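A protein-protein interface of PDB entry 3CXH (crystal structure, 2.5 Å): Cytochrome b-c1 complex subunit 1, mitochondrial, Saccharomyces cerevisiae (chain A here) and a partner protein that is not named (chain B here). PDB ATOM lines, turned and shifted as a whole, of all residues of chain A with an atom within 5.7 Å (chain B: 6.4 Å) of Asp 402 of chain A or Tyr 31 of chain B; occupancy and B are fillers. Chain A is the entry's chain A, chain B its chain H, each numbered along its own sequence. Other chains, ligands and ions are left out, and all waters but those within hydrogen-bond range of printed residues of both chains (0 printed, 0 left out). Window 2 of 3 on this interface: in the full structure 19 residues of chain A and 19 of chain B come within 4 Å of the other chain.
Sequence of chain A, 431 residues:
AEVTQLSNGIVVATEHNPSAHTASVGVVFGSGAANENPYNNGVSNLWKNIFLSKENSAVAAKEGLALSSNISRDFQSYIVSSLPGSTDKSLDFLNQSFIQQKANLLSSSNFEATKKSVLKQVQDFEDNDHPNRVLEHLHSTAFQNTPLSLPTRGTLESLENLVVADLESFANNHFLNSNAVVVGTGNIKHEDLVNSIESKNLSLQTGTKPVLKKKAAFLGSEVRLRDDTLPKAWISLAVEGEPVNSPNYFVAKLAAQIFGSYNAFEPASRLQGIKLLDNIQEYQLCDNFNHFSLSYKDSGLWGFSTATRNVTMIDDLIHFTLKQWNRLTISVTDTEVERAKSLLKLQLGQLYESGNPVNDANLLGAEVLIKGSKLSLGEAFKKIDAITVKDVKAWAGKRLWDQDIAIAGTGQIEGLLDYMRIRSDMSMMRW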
ATOM      1  N   LEU A 400       5.787  32.471  -9.114  1.00  0.00           N
ATOM      2  CA  LEU A 400       5.014  31.232  -9.061  1.00  0.00           C
ATOM      3  C   LEU A 400       4.398  30.698 -10.351  1.00  0.00           C
ATOM      4  O   LEU A 400       4.608  29.536 -10.714  1.00  0.00           O
ATOM      5  CB  LEU A 400       3.914  31.403  -8.021  1.00  0.00           C
ATOM      6  CG  LEU A 400       3.880  30.513  -6.783  1.00  0.00           C
ATOM      7  CD1 LEU A 400       5.206  29.830  -6.528  1.00  0.00           C
ATOM      8  CD2 LEU A 400       3.451  31.361  -5.612  1.00  0.00           C
ATOM      9  N   TRP A 401       3.636  31.543 -11.034  1.00  0.00           N
ATOM     10  CA  TRP A 401       2.958  31.148 -12.259  1.00  0.00           C
ATOM     11  C   TRP A 401       3.836  30.587 -13.374  1.00  0.00           C
ATOM     12  O   TRP A 401       4.638  31.303 -13.964  1.00  0.00           O
ATOM     13  CB  TRP A 401       2.124  32.311 -12.794  1.00  0.00           C
ATOM     14  CG  TRP A 401       1.146  31.901 -13.862  1.00  0.00           C
ATOM     15  CD1 TRP A 401       1.360  31.882 -15.212  1.00  0.00           C
ATOM     16  CD2 TRP A 401      -0.201  31.454 -13.663  1.00  0.00           C
ATOM     17  NE1 TRP A 401       0.229  31.452 -15.864  1.00  0.00           N
ATOM     18  CE2 TRP A 401      -0.744  31.185 -14.938  1.00  0.00           C
ATOM     19  CE3 TRP A 401      -1.002  31.256 -12.528  1.00  0.00           C
ATOM     20  CZ2 TRP A 401      -2.052  30.730 -15.112  1.00  0.00           C
ATOM     21  CZ3 TRP A 401      -2.300  30.806 -12.701  1.00  0.00           C
ATOM     22  CH2 TRP A 401      -2.814  30.548 -13.985  1.00  0.00           C
ATOM     23  N   ASP A 402       3.660  29.300 -13.666  1.00  0.00           N
ATOM     24  CA  ASP A 402       4.397  28.640 -14.731  1.00  0.00           C
ATOM     25  C   ASP A 402       5.911  28.818 -14.609  1.00  0.00           C
ATOM     26  O   ASP A 402       6.579  29.216 -15.561  1.00  0.00           O
ATOM     27  CB  ASP A 402       3.895  29.152 -16.092  1.00  0.00           C
ATOM     28  CG  ASP A 402       4.426  28.342 -17.272  1.00  0.00           C
ATOM     29  OD1 ASP A 402       4.728  27.138 -17.122  1.00  0.00           O
ATOM     30  OD2 ASP A 402       4.528  28.916 -18.372  1.00  0.00           O
ATOM     31  N   GLN A 403       6.440  28.534 -13.424  1.00  0.00           N
ATOM     32  CA  GLN A 403       7.874  28.624 -13.165  1.00  0.00           C
ATOM     33  C   GLN A 403       8.439  27.263 -12.769  1.00  0.00           C
ATOM     34  O   GLN A 403       7.701  26.392 -12.297  1.00  0.00           O
ATOM     35  CB  GLN A 403       8.165  29.653 -12.065  1.00  0.00           C
ATOM     36  CG  GLN A 403       7.947  31.111 -12.486  1.00  0.00           C
ATOM     37  CD  GLN A 403       9.027  31.652 -13.417  1.00  0.00           C
ATOM     38  OE1 GLN A 403       9.433  32.798 -13.291  1.00  0.00           O
ATOM     39  NE2 GLN A 403       9.480  30.838 -14.358  1.00  0.00           N
ATOM     40  N   ASP A 404       9.738  27.071 -12.997  1.00  0.00           N
ATOM     41  CA  ASP A 404      10.409  25.822 -12.657  1.00  0.00           C
ATOM     42  C   ASP A 404      10.363  25.585 -11.156  1.00  0.00           C
ATOM     43  O   ASP A 404      10.293  26.527 -10.367  1.00  0.00           O
ATOM     44  CB  ASP A 404      11.863  25.847 -13.125  1.00  0.00           C
ATOM     45  CG  ASP A 404      12.049  25.249 -14.514  1.00  0.00           C
ATOM     46  OD1 ASP A 404      13.075  25.566 -15.167  1.00  0.00           O
ATOM     47  OD2 ASP A 404      11.194  24.442 -14.942  1.00  0.00           O
ATOM     48  N   MET A 420       7.586  16.642 -14.832  1.00  0.00           N
ATOM     49  CA  MET A 420       6.680  17.335 -15.747  1.00  0.00           C
ATOM     50  C   MET A 420       5.219  17.403 -15.328  1.00  0.00           C
ATOM     51  O   MET A 420       4.551  18.407 -15.578  1.00  0.00           O
ATOM     52  CB  MET A 420       6.825  16.791 -17.163  1.00  0.00           C
ATOM     53  CG  MET A 420       8.076  17.312 -17.861  1.00  0.00           C
ATOM     54  SD  MET A 420       8.192  19.133 -17.750  1.00  0.00           S
ATOM     55  CE  MET A 420       7.002  19.604 -18.968  1.00  0.00           C
ATOM     56  N   ARG A 423       5.250  19.865 -12.520  1.00  0.00           N
ATOM     57  CA  ARG A 423       5.563  21.130 -13.181  1.00  0.00           C
ATOM     58  C   ARG A 423       4.369  21.747 -13.912  1.00  0.00           C
ATOM     59  O   ARG A 423       4.164  22.958 -13.843  1.00  0.00           O
ATOM     60  CB  ARG A 423       6.765  20.948 -14.123  1.00  0.00           C
ATOM     61  CG  ARG A 423       7.092  22.150 -15.002  1.00  0.00           C
ATOM     62  CD  ARG A 423       7.304  23.426 -14.192  1.00  0.00           C
ATOM     63  NE  ARG A 423       6.812  24.590 -14.928  1.00  0.00           N
ATOM     64  CZ  ARG A 423       7.593  25.419 -15.600  1.00  0.00           C
ATOM     65  NH1 ARG A 423       7.076  26.439 -16.255  1.00  0.00           N
ATOM     66  NH2 ARG A 423       8.899  25.246 -15.583  1.00  0.00           N
ATOM     67  N   MET A 426       1.851  24.231 -12.275  1.00  0.00           N
ATOM     68  CA  MET A 426       2.260  25.582 -11.885  1.00  0.00           C
ATOM     69  C   MET A 426       1.427  26.658 -12.563  1.00  0.00           C
ATOM     70  O   MET A 426       1.607  27.842 -12.306  1.00  0.00           O
ATOM     71  CB  MET A 426       3.747  25.824 -12.134  1.00  0.00           C
ATOM     72  CG  MET A 426       4.684  24.976 -11.274  1.00  0.00           C
ATOM     73  SD  MET A 426       4.327  25.034  -9.502  1.00  0.00           S
ATOM     74  CE  MET A 426       4.842  26.696  -9.120  1.00  0.00           C
ATOM     75  N   SER A 427       0.488  26.239 -13.402  1.00  0.00           N
ATOM     76  CA  SER A 427      -0.390  27.166 -14.105  1.00  0.00           C
ATOM     77  C   SER A 427      -1.715  26.499 -14.444  1.00  0.00           C
ATOM     78  O   SER A 427      -1.866  25.292 -14.293  1.00  0.00           O
ATOM     79  CB  SER A 427       0.273  27.663 -15.389  1.00  0.00           C
ATOM     80  OG  SER A 427       0.548  26.592 -16.272  1.00  0.00           O
ATOM     81  N   VAL B  28      16.638  17.015 -14.285  1.00  0.00           N
ATOM     82  CA  VAL B  28      16.614  18.453 -14.499  1.00  0.00           C
ATOM     83  C   VAL B  28      15.412  18.819 -15.365  1.00  0.00           C
ATOM     84  O   VAL B  28      15.008  18.058 -16.241  1.00  0.00           O
ATOM     85  CB  VAL B  28      17.921  18.937 -15.161  1.00  0.00           C
ATOM     86  CG1 VAL B  28      17.749  20.349 -15.694  1.00  0.00           C
ATOM     87  CG2 VAL B  28      19.064  18.903 -14.133  1.00  0.00           C
ATOM     88  N   SER B  29      14.814  19.968 -15.080  1.00  0.00           N
ATOM     89  CA  SER B  29      13.669  20.434 -15.834  1.00  0.00           C
ATOM     90  C   SER B  29      13.996  20.614 -17.304  1.00  0.00           C
ATOM     91  O   SER B  29      15.091  21.044 -17.661  1.00  0.00           O
ATOM     92  CB  SER B  29      13.178  21.771 -15.293  1.00  0.00           C
ATOM     93  OG  SER B  29      12.257  22.350 -16.202  1.00  0.00           O
ATOM     94  N   PRO B  30      13.049  20.251 -18.180  1.00  0.00           N
ATOM     95  CA  PRO B  30      13.200  20.372 -19.633  1.00  0.00           C
ATOM     96  C   PRO B  30      13.343  21.844 -20.023  1.00  0.00           C
ATOM     97  O   PRO B  30      13.931  22.180 -21.048  1.00  0.00           O
ATOM     98  CB  PRO B  30      11.884  19.793 -20.148  1.00  0.00           C
ATOM     99  CG  PRO B  30      11.576  18.738 -19.129  1.00  0.00           C
ATOM    100  CD  PRO B  30      11.854  19.455 -17.841  1.00  0.00           C
ATOM    101  N   TYR B  31      12.797  22.716 -19.183  1.00  0.00           N
ATOM    102  CA  TYR B  31      12.845  24.155 -19.413  1.00  0.00           C
ATOM    103  C   TYR B  31      14.248  24.711 -19.259  1.00  0.00           C
ATOM    104  O   TYR B  31      14.555  25.769 -19.807  1.00  0.00           O
ATOM    105  CB  TYR B  31      11.916  24.882 -18.444  1.00  0.00           C
ATOM    106  CG  TYR B  31      10.447  24.815 -18.794  1.00  0.00           C
ATOM    107  CD1 TYR B  31       9.648  23.757 -18.352  1.00  0.00           C
ATOM    108  CD2 TYR B  31       9.841  25.844 -19.509  1.00  0.00           C
ATOM    109  CE1 TYR B  31       8.282  23.735 -18.607  1.00  0.00           C
ATOM    110  CE2 TYR B  31       8.474  25.830 -19.769  1.00  0.00           C
ATOM    111  CZ  TYR B  31       7.699  24.776 -19.311  1.00  0.00           C
ATOM    112  OH  TYR B  31       6.341  24.799 -19.529  1.00  0.00           O
ATOM    113  N   ALA B  32      15.085  24.007 -18.497  1.00  0.00           N
ATOM    114  CA  ALA B  32      16.460  24.427 -18.255  1.00  0.00           C
ATOM    115  C   ALA B  32      17.477  23.683 -19.115  1.00  0.00           C
ATOM    116  O   ALA B  32      18.682  23.783 -18.888  1.00  0.00           O
ATOM    117  CB  ALA B  32      16.802  24.266 -16.785  1.00  0.00           C
ATOM    118  N   GLN B  33      16.996  22.929 -20.094  1.00  0.00           N
ATOM    119  CA  GLN B  33      17.883  22.180 -20.970  1.00  0.00           C
ATOM    120  C   GLN B  33      18.066  22.859 -22.309  1.00  0.00           C
ATOM    121  O   GLN B  33      17.251  23.690 -22.713  1.00  0.00           O
ATOM    122  CB  GLN B  33      17.375  20.753 -21.171  1.00  0.00           C
ATOM    123  CG  GLN B  33      17.503  19.897 -19.930  1.00  0.00           C
ATOM    124  CD  GLN B  33      17.058  18.472 -20.149  1.00  0.00           C
ATOM    125  OE1 GLN B  33      17.423  17.839 -21.139  1.00  0.00           O
ATOM    126  NE2 GLN B  33      16.275  17.949 -19.215  1.00  0.00           N
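OD2 of Asp 404 of chain A lies within hydrogen-bond range of OG of Ser 29 of chain B, 2.7 Å away.
OD1 of Asp 402 of chain A lies within salt-bridge range of NH1 of Arg 423 of chain A, at 2.6 Å. The backbone NH of Asp 402 of chain A sits at hydrogen-bond distance from the backbone carbonyl oxygen of Met 426 of chain A. The backbone carbonyl oxygen (O) of Gln 403 of chain A lies within hydrogen-bond range of the guanidinium group (NE) of Arg 423 of chain A. OD2 of Asp 404 of chain A is in salt-bridge range of NH2 of Arg 423 of chain A (2.5 Å). The backbone NH (N) of Tyr 31 of chain B sits at hydrogen-bond distance from the side-chain hydroxyl (OG) of Ser 29 of chain B (3.1 Å).
Tyr 31 of chain B touches Asp 402 of chain A (OH to OD1, 3.7 Å). Asp 404 of chain A touches Tyr 31 of chain B. Met 420 of chain A touches Pro 30 of chain B (SD to CG, 3.7 Å). NH2 of Arg 423 of chain A touches CD1 of Tyr 31 of chain B, at 3.2 Å.
Asp 402 of chain A touches just one residue of chain B: Tyr 31. Tyr 31 of chain B touches just these residues of chain A: Asp 402, Asp 404 and Arg 423. Of the printed residues of chain A, Ser 29 of chain B touches Asp 404 (2.7 Å). Of the printed residues of chain B, Asp 404 of chain A touches Ser 29 and Tyr 31. Printed residues of chain A within 4 Å of Pro 30 of chain B: Met 420. Val 28 of chain B touches none of the printed residues of chain A. The nearest printed residue of chain B that does not touch Asp 402 of chain A is Ser 29 of chain B (8.9 Å).
Of the 9 printed residues of chain A, 4 touch a printed residue of chain B. Hydrophobic or aromatic side chains of chain A that line the printed part of chain B: Met 420. Along chain B the printed residues that touch a printed residue of chain A span positions 29 to 31. Among the printed residues, no Asp or Glu carboxylate lies within 4 Å of a Lys or Arg side-chain nitrogen of the other chain.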
